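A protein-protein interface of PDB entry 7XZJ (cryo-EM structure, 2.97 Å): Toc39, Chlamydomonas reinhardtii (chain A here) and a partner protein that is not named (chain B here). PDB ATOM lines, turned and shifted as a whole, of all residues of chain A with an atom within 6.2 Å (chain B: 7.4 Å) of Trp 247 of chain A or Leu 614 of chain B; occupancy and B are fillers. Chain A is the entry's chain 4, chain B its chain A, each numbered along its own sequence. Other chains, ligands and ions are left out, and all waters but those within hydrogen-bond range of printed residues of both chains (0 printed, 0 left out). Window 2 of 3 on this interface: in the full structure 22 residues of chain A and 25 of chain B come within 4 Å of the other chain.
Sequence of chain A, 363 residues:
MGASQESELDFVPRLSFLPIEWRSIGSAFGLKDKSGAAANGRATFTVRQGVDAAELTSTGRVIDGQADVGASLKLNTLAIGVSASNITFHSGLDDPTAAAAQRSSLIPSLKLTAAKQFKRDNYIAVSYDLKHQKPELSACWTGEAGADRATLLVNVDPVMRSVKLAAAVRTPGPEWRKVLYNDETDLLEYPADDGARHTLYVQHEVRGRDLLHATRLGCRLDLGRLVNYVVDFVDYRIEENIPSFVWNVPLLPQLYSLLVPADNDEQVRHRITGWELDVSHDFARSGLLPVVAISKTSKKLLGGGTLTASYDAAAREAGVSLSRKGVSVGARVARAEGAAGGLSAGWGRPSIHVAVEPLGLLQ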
ATOM      1  N   GLU A 239     -10.079  17.528 -25.556  1.00  0.00           N
ATOM      2  CA  GLU A 239      -9.631  16.238 -24.954  1.00  0.00           C
ATOM      3  C   GLU A 239      -8.170  15.930 -25.308  1.00  0.00           C
ATOM      4  O   GLU A 239      -7.436  15.491 -24.402  1.00  0.00           O
ATOM      5  CB  GLU A 239     -10.561  15.095 -25.369  1.00  0.00           C
ATOM      6  CG  GLU A 239     -10.495  13.887 -24.449  1.00  0.00           C
ATOM      7  CD  GLU A 239      -9.372  12.902 -24.730  1.00  0.00           C
ATOM      8  OE1 GLU A 239      -8.943  12.811 -25.898  1.00  0.00           O
ATOM      9  OE2 GLU A 239      -8.922  12.238 -23.777  1.00  0.00           O
ATOM     10  N   ILE A 242      -5.892  17.872 -23.114  1.00  0.00           N
ATOM     11  CA  ILE A 242      -5.946  17.548 -21.655  1.00  0.00           C
ATOM     12  C   ILE A 242      -4.860  16.525 -21.302  1.00  0.00           C
ATOM     13  O   ILE A 242      -4.725  15.526 -22.035  1.00  0.00           O
ATOM     14  CB  ILE A 242      -7.355  17.048 -21.271  1.00  0.00           C
ATOM     15  CG1 ILE A 242      -8.403  18.154 -21.417  1.00  0.00           C
ATOM     16  CG2 ILE A 242      -7.377  16.453 -19.871  1.00  0.00           C
ATOM     17  N   PRO A 243      -4.089  16.732 -20.207  1.00  0.00           N
ATOM     18  CA  PRO A 243      -3.059  15.780 -19.769  1.00  0.00           C
ATOM     19  C   PRO A 243      -3.625  14.474 -19.200  1.00  0.00           C
ATOM     20  O   PRO A 243      -4.806  14.428 -18.919  1.00  0.00           O
ATOM     21  CB  PRO A 243      -2.323  16.516 -18.639  1.00  0.00           C
ATOM     22  CG  PRO A 243      -2.695  17.969 -18.827  1.00  0.00           C
ATOM     23  CD  PRO A 243      -4.107  17.930 -19.368  1.00  0.00           C
ATOM     24  N   SER A 244      -2.768  13.468 -19.005  1.00  0.00           N
ATOM     25  CA  SER A 244      -3.226  12.164 -18.540  1.00  0.00           C
ATOM     26  C   SER A 244      -3.317  12.072 -17.023  1.00  0.00           C
ATOM     27  O   SER A 244      -4.141  11.306 -16.502  1.00  0.00           O
ATOM     28  CB  SER A 244      -2.293  11.068 -19.060  1.00  0.00           C
ATOM     29  OG  SER A 244      -0.987  11.214 -18.528  1.00  0.00           O
ATOM     30  N   PHE A 245      -2.479  12.825 -16.303  1.00  0.00           N
ATOM     31  CA  PHE A 245      -2.517  12.788 -14.845  1.00  0.00           C
ATOM     32  C   PHE A 245      -3.879  13.208 -14.314  1.00  0.00           C
ATOM     33  O   PHE A 245      -4.281  12.779 -13.226  1.00  0.00           O
ATOM     34  CB  PHE A 245      -1.421  13.683 -14.267  1.00  0.00           C
ATOM     35  N   VAL A 246      -4.601  14.043 -15.062  1.00  0.00           N
ATOM     36  CA  VAL A 246      -5.978  14.356 -14.698  1.00  0.00           C
ATOM     37  C   VAL A 246      -6.860  13.125 -14.852  1.00  0.00           C
ATOM     38  O   VAL A 246      -7.696  12.833 -13.989  1.00  0.00           O
ATOM     39  CB  VAL A 246      -6.496  15.537 -15.537  1.00  0.00           C
ATOM     40  N   TRP A 247      -6.683  12.375 -15.944  1.00  0.00           N
ATOM     41  CA  TRP A 247      -7.451  11.152 -16.138  1.00  0.00           C
ATOM     42  C   TRP A 247      -7.110  10.092 -15.104  1.00  0.00           C
ATOM     43  O   TRP A 247      -7.894   9.157 -14.905  1.00  0.00           O
ATOM     44  CB  TRP A 247      -7.223  10.597 -17.545  1.00  0.00           C
ATOM     45  CG  TRP A 247      -7.612  11.548 -18.630  1.00  0.00           C
ATOM     46  CD1 TRP A 247      -6.794  12.093 -19.574  1.00  0.00           C
ATOM     47  CD2 TRP A 247      -8.920  12.077 -18.879  1.00  0.00           C
ATOM     48  NE1 TRP A 247      -7.510  12.923 -20.400  1.00  0.00           N
ATOM     49  CE2 TRP A 247      -8.819  12.931 -19.993  1.00  0.00           C
ATOM     50  CE3 TRP A 247     -10.165  11.907 -18.268  1.00  0.00           C
ATOM     51  CZ2 TRP A 247      -9.915  13.616 -20.508  1.00  0.00           C
ATOM     52  CZ3 TRP A 247     -11.252  12.587 -18.781  1.00  0.00           C
ATOM     53  CH2 TRP A 247     -11.121  13.431 -19.891  1.00  0.00           C
ATOM     54  N   ASN A 248      -5.952  10.211 -14.450  1.00  0.00           N
ATOM     55  CA  ASN A 248      -5.604   9.286 -13.376  1.00  0.00           C
ATOM     56  C   ASN A 248      -6.603   9.327 -12.225  1.00  0.00           C
ATOM     57  O   ASN A 248      -6.684   8.361 -11.459  1.00  0.00           O
ATOM     58  CB  ASN A 248      -4.200   9.593 -12.852  1.00  0.00           C
ATOM     59  CG  ASN A 248      -3.126   9.375 -13.898  1.00  0.00           C
ATOM     60  OD1 ASN A 248      -3.418   9.058 -15.051  1.00  0.00           O
ATOM     61  ND2 ASN A 248      -1.872   9.551 -13.501  1.00  0.00           N
ATOM     62  N   VAL A 249      -7.355  10.416 -12.085  1.00  0.00           N
ATOM     63  CA  VAL A 249      -8.313  10.557 -10.981  1.00  0.00           C
ATOM     64  C   VAL A 249      -9.389   9.484 -11.100  1.00  0.00           C
ATOM     65  O   VAL A 249      -9.938   9.277 -12.200  1.00  0.00           O
ATOM     66  CB  VAL A 249      -8.936  11.965 -10.988  1.00  0.00           C
ATOM     67  CG1 VAL A 249     -10.048  12.070  -9.956  1.00  0.00           C
ATOM     68  CG2 VAL A 249      -7.867  13.017 -10.734  1.00  0.00           C
ATOM     69  N   PRO A 250      -9.724   8.771 -10.024  1.00  0.00           N
ATOM     70  CA  PRO A 250     -10.740   7.715 -10.128  1.00  0.00           C
ATOM     71  C   PRO A 250     -12.129   8.278 -10.395  1.00  0.00           C
ATOM     72  O   PRO A 250     -12.497   9.341  -9.888  1.00  0.00           O
ATOM     73  CB  PRO A 250     -10.675   7.026  -8.762  1.00  0.00           C
ATOM     74  CG  PRO A 250     -10.143   8.074  -7.842  1.00  0.00           C
ATOM     75  CD  PRO A 250      -9.172   8.873  -8.663  1.00  0.00           C
ATOM     76  N   LEU A 252     -13.428   9.813 -12.585  1.00  0.00           N
ATOM     77  CA  LEU A 252     -13.518  10.959 -13.487  1.00  0.00           C
ATOM     78  C   LEU A 252     -13.818  10.556 -14.925  1.00  0.00           C
ATOM     79  O   LEU A 252     -14.673  11.204 -15.555  1.00  0.00           O
ATOM     80  CB  LEU A 252     -12.235  11.793 -13.396  1.00  0.00           C
ATOM     81  CG  LEU A 252     -12.136  12.968 -14.371  1.00  0.00           C
ATOM     82  CD1 LEU A 252     -13.291  13.937 -14.166  1.00  0.00           C
ATOM     83  CD2 LEU A 252     -10.802  13.683 -14.223  1.00  0.00           C
ATOM     84  N   PRO A 253     -13.160   9.548 -15.517  1.00  0.00           N
ATOM     85  CA  PRO A 253     -13.496   9.194 -16.908  1.00  0.00           C
ATOM     86  C   PRO A 253     -14.947   8.786 -17.105  1.00  0.00           C
ATOM     87  O   PRO A 253     -15.522   9.081 -18.157  1.00  0.00           O
ATOM     88  CB  PRO A 253     -12.531   8.041 -17.216  1.00  0.00           C
ATOM     89  CG  PRO A 253     -11.394   8.249 -16.293  1.00  0.00           C
ATOM     90  CD  PRO A 253     -12.003   8.770 -15.033  1.00  0.00           C
ATOM     91  N   TYR A 256     -16.910  11.925 -17.260  1.00  0.00           N
ATOM     92  CA  TYR A 256     -16.637  12.569 -18.540  1.00  0.00           C
ATOM     93  C   TYR A 256     -17.396  11.891 -19.674  1.00  0.00           C
ATOM     94  O   TYR A 256     -17.925  12.562 -20.568  1.00  0.00           O
ATOM     95  CB  TYR A 256     -15.137  12.563 -18.820  1.00  0.00           C
ATOM     96  CG  TYR A 256     -14.768  13.201 -20.136  1.00  0.00           C
ATOM     97  CD1 TYR A 256     -14.655  14.580 -20.252  1.00  0.00           C
ATOM     98  CD2 TYR A 256     -14.527  12.428 -21.263  1.00  0.00           C
ATOM     99  CE1 TYR A 256     -14.317  15.169 -21.450  1.00  0.00           C
ATOM    100  CE2 TYR A 256     -14.188  13.008 -22.466  1.00  0.00           C
ATOM    101  CZ  TYR A 256     -14.085  14.379 -22.553  1.00  0.00           C
ATOM    102  OH  TYR A 256     -13.748  14.965 -23.750  1.00  0.00           O
ATOM    103  N   ILE B 611     -14.928   3.129 -31.353  1.00  0.00           N
ATOM    104  CA  ILE B 611     -14.020   2.737 -30.281  1.00  0.00           C
ATOM    105  C   ILE B 611     -14.111   3.728 -29.124  1.00  0.00           C
ATOM    106  O   ILE B 611     -14.477   4.895 -29.288  1.00  0.00           O
ATOM    107  CB  ILE B 611     -12.577   2.614 -30.796  1.00  0.00           C
ATOM    108  CG1 ILE B 611     -12.058   3.973 -31.261  1.00  0.00           C
ATOM    109  CG2 ILE B 611     -12.504   1.608 -31.926  1.00  0.00           C
ATOM    110  CD1 ILE B 611     -10.730   3.901 -31.969  1.00  0.00           C
ATOM    111  N   GLN B 612     -13.763   3.243 -27.931  1.00  0.00           N
ATOM    112  CA  GLN B 612     -13.767   4.036 -26.701  1.00  0.00           C
ATOM    113  C   GLN B 612     -12.385   3.948 -26.067  1.00  0.00           C
ATOM    114  O   GLN B 612     -12.128   3.061 -25.237  1.00  0.00           O
ATOM    115  CB  GLN B 612     -14.847   3.548 -25.737  1.00  0.00           C
ATOM    116  N   PRO B 613     -11.460   4.839 -26.434  1.00  0.00           N
ATOM    117  CA  PRO B 613     -10.104   4.764 -25.867  1.00  0.00           C
ATOM    118  C   PRO B 613     -10.058   4.928 -24.359  1.00  0.00           C
ATOM    119  O   PRO B 613      -9.179   4.347 -23.711  1.00  0.00           O
ATOM    120  CB  PRO B 613      -9.366   5.905 -26.582  1.00  0.00           C
ATOM    121  CG  PRO B 613     -10.444   6.846 -27.008  1.00  0.00           C
ATOM    122  CD  PRO B 613     -11.617   5.980 -27.352  1.00  0.00           C
ATOM    123  N   LEU B 614     -10.972   5.700 -23.777  1.00  0.00           N
ATOM    124  CA  LEU B 614     -10.982   5.943 -22.341  1.00  0.00           C
ATOM    125  C   LEU B 614     -11.772   4.895 -21.568  1.00  0.00           C
ATOM    126  O   LEU B 614     -12.033   5.088 -20.377  1.00  0.00           O
ATOM    127  CB  LEU B 614     -11.537   7.337 -22.040  1.00  0.00           C
ATOM    128  CG  LEU B 614     -10.623   8.529 -22.338  1.00  0.00           C
ATOM    129  CD1 LEU B 614     -10.722   8.960 -23.795  1.00  0.00           C
ATOM    130  CD2 LEU B 614     -10.937   9.690 -21.407  1.00  0.00           C
ATOM    131  N   GLN B 615     -12.167   3.800 -22.219  1.00  0.00           N
ATOM    132  CA  GLN B 615     -12.924   2.760 -21.529  1.00  0.00           C
ATOM    133  C   GLN B 615     -12.072   2.053 -20.480  1.00  0.00           C
ATOM    134  O   GLN B 615     -12.523   1.822 -19.352  1.00  0.00           O
ATOM    135  CB  GLN B 615     -13.474   1.757 -22.542  1.00  0.00           C
ATOM    136  N   ASN B 616     -10.838   1.698 -20.833  1.00  0.00           N
ATOM    137  CA  ASN B 616      -9.989   0.871 -19.989  1.00  0.00           C
ATOM    138  C   ASN B 616      -8.622   1.520 -19.818  1.00  0.00           C
ATOM    139  O   ASN B 616      -8.150   2.249 -20.694  1.00  0.00           O
ATOM    140  CB  ASN B 616      -9.830  -0.538 -20.579  1.00  0.00           C
ATOM    141  CG  ASN B 616      -8.950  -1.431 -19.731  1.00  0.00           C
ATOM    142  OD1 ASN B 616      -7.730  -1.453 -19.893  1.00  0.00           O
ATOM    143  ND2 ASN B 616      -9.565  -2.172 -18.816  1.00  0.00           N
ATOM    144  N   GLY B 617      -7.990   1.238 -18.675  1.00  0.00           N
ATOM    145  CA  GLY B 617      -6.694   1.830 -18.386  1.00  0.00           C
ATOM    146  C   GLY B 617      -5.619   1.434 -19.382  1.00  0.00           C
ATOM    147  O   GLY B 617      -4.829   2.273 -19.822  1.00  0.00           O
ATOM    148  N   THR B 619      -6.153   0.416 -22.471  1.00  0.00           N
ATOM    149  CA  THR B 619      -6.526   1.134 -23.682  1.00  0.00           C
ATOM    150  C   THR B 619      -6.106   2.593 -23.589  1.00  0.00           C
ATOM    151  O   THR B 619      -5.594   3.166 -24.558  1.00  0.00           O
ATOM    152  CB  THR B 619      -8.032   1.020 -23.911  1.00  0.00           C
ATOM    153  OG1 THR B 619      -8.453  -0.321 -23.635  1.00  0.00           O
ATOM    154  CG2 THR B 619      -8.378   1.362 -25.349  1.00  0.00           C
ATOM    155  N   ARG B 620      -6.294   3.202 -22.416  1.00  0.00           N
ATOM    156  CA  ARG B 620      -5.913   4.598 -22.233  1.00  0.00           C
ATOM    157  C   ARG B 620      -4.418   4.794 -22.438  1.00  0.00           C
ATOM    158  O   ARG B 620      -3.995   5.745 -23.098  1.00  0.00           O
ATOM    159  CB  ARG B 620      -6.325   5.082 -20.843  1.00  0.00           C
ATOM    160  CG  ARG B 620      -7.802   5.380 -20.695  1.00  0.00           C
ATOM    161  CD  ARG B 620      -8.056   6.317 -19.526  1.00  0.00           C
ATOM    162  NE  ARG B 620      -7.469   5.826 -18.289  1.00  0.00           N
ATOM    163  CZ  ARG B 620      -8.085   5.016 -17.436  1.00  0.00           C
ATOM    164  NH1 ARG B 620      -9.308   4.567 -17.670  1.00  0.00           N
ATOM    165  NH2 ARG B 620      -7.461   4.651 -16.321  1.00  0.00           N
ATOM    166  N   TYR B 623      -3.518   4.405 -26.025  1.00  0.00           N
ATOM    167  CA  TYR B 623      -3.996   5.610 -26.748  1.00  0.00           C
ATOM    168  C   TYR B 623      -3.026   6.760 -26.475  1.00  0.00           C
ATOM    169  O   TYR B 623      -2.689   7.499 -27.418  1.00  0.00           O
ATOM    170  CB  TYR B 623      -5.418   5.955 -26.298  1.00  0.00           C
ATOM    171  CG  TYR B 623      -5.899   7.331 -26.681  1.00  0.00           C
ATOM    172  CD1 TYR B 623      -6.112   7.670 -28.007  1.00  0.00           C
ATOM    173  CD2 TYR B 623      -6.158   8.291 -25.718  1.00  0.00           C
ATOM    174  CE1 TYR B 623      -6.558   8.930 -28.368  1.00  0.00           C
ATOM    175  CE2 TYR B 623      -6.606   9.555 -26.060  1.00  0.00           C
ATOM    176  CZ  TYR B 623      -6.807   9.877 -27.390  1.00  0.00           C
ATOM    177  OH  TYR B 623      -7.248  11.121 -27.737  1.00  0.00           O
ATOM    178  N   GLN B 624      -2.576   6.884 -25.225  1.00  0.00           N
ATOM    179  CA  GLN B 624      -1.665   7.995 -24.849  1.00  0.00           C
ATOM    180  C   GLN B 624      -0.367   7.864 -25.644  1.00  0.00           C
ATOM    181  O   GLN B 624       0.098   8.881 -26.179  1.00  0.00           O
ATOM    182  CB  GLN B 624      -1.379   7.956 -23.347  1.00  0.00           C
ATOM    183  CG  GLN B 624      -0.567   9.143 -22.850  1.00  0.00           C
ATOM    184  CD  GLN B 624      -1.344  10.434 -22.924  1.00  0.00           C
ATOM    185  OE1 GLN B 624      -2.562  10.459 -22.765  1.00  0.00           O
ATOM    186  NE2 GLN B 624      -0.635  11.527 -23.157  1.00  0.00           N
ATOM    187  N   ARG B 627      -0.781   8.915 -29.102  1.00  0.00           N
ATOM    188  CA  ARG B 627      -1.081  10.368 -29.144  1.00  0.00           C
ATOM    189  C   ARG B 627       0.239  11.133 -29.035  1.00  0.00           C
ATOM    190  O   ARG B 627       0.419  12.102 -29.786  1.00  0.00           O
ATOM    191  CB  ARG B 627      -2.049  10.747 -28.020  1.00  0.00           C
ATOM    192  CG  ARG B 627      -2.716  12.102 -28.203  1.00  0.00           C
ATOM    193  CD  ARG B 627      -3.871  12.337 -27.249  1.00  0.00           C
ATOM    194  NE  ARG B 627      -3.460  12.526 -25.866  1.00  0.00           N
ATOM    195  CZ  ARG B 627      -4.295  12.778 -24.864  1.00  0.00           C
ATOM    196  NH1 ARG B 627      -5.594  12.868 -25.092  1.00  0.00           N
ATOM    197  NH2 ARG B 627      -3.830  12.941 -23.639  1.00  0.00           N
ATOM    198  N   TYR B1048      -5.783   0.974 -31.636  1.00  0.00           N
ATOM    199  CA  TYR B1048      -4.728   1.935 -31.333  1.00  0.00           C
ATOM    200  C   TYR B1048      -3.418   1.223 -31.057  1.00  0.00           C
ATOM    201  O   TYR B1048      -2.385   1.561 -31.652  1.00  0.00           O
ATOM    202  CB  TYR B1048      -5.116   2.796 -30.132  1.00  0.00           C
ATOM    203  CG  TYR B1048      -5.927   4.023 -30.467  1.00  0.00           C
ATOM    204  CD1 TYR B1048      -5.390   5.045 -31.236  1.00  0.00           C
ATOM    205  CD2 TYR B1048      -7.220   4.172 -29.988  1.00  0.00           C
ATOM    206  CE1 TYR B1048      -6.124   6.169 -31.534  1.00  0.00           C
ATOM    207  CE2 TYR B1048      -7.959   5.292 -30.279  1.00  0.00           C
ATOM    208  CZ  TYR B1048      -7.407   6.286 -31.052  1.00  0.00           C
ATOM    209  OH  TYR B1048      -8.151   7.403 -31.339  1.00  0.00           O
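OE1 of Glu 239 of chain A lies within hydrogen-bond range of OH of Tyr 623 of chain B, at 3.0 Å. OE1 of Glu 239 of chain A is in salt-bridge range of NH1 of Arg 627 of chain B (3.4 Å). O of Ile 242 of chain A lies within hydrogen-bond range of NH2 of Arg 627 of chain B.
O of Pro 243 of chain A lies close to NE1 of Trp 247 of chain A. The side-chain amide oxygen (OD1) of Asn 248 of chain A sits close to the backbone carbonyl oxygen (O) of Ser 244 of chain A, 2.8 Å away. OE1 of Gln 624 of chain B lies within hydrogen-bond range of NH2 of Arg 627 of chain B (2.9 Å).
OE2 of Glu 239 of chain A touches CD1 of Leu 614 of chain B, at 3.7 Å. Ser 244 of chain A touches Gln 624 of chain B. CD2 of Leu 614 of chain B touches CE3 of Trp 247 of chain A, 3.9 Å away.
Printed residues of chain B within 4 Å of Glu 239 of chain A: Leu 614 (3.7 Å), Tyr 623 (3.0 Å) and Arg 627 (3.3 Å). Of the printed residues of chain B, Ile 242 of chain A touches Arg 627. Of the printed residues of chain B, Ser 244 of chain A touches Gln 624. No residue of chain B comes within 4 Å of Val 246 of chain A. Trp 247 of chain A touches just one residue of chain B: Leu 614 (3.9 Å). Pro 253 of chain A touches none of the printed residues of chain B. Ile 611 of chain B touches none of the printed residues of chain A. Leu 614 of chain B touches just these residues of chain A: Glu 239 (3.7 Å) and Trp 247 (3.9 Å). Of the printed residues of chain A, Arg 627 of chain B touches Glu 239 (3.3 Å) and Ile 242 (3.2 Å). The nearest residue of chain B that does not touch Trp 247 of chain A is Arg 620 of chain B (4.7 Å). The nearest residue of chain A that does not touch Leu 614 of chain B is Pro 253 of chain A (4.4 Å). The nearest printed residue of chain A that does not touch Arg 627 of chain B is Pro 243 of chain A (4.7 Å).
Of the 13 printed residues of chain B, 4 touch a printed residue of chain A. Printed residues of chain B that touch a printed residue of chain A: Leu 614, Tyr 623, Gln 624 and Arg 627. Hydrophobic or aromatic side chains of chain B within 4 Å of the printed part of chain A: Leu 614 and Tyr 623. Hydrophobic or aromatic side chains of chain A that line the printed part of chain B: Trp 247. Among the printed residues, Asp or Glu carboxylates within 4 Å of a Lys or Arg side-chain nitrogen of the other chain: Glu 239 of chain A with Arg 627 of chain B.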
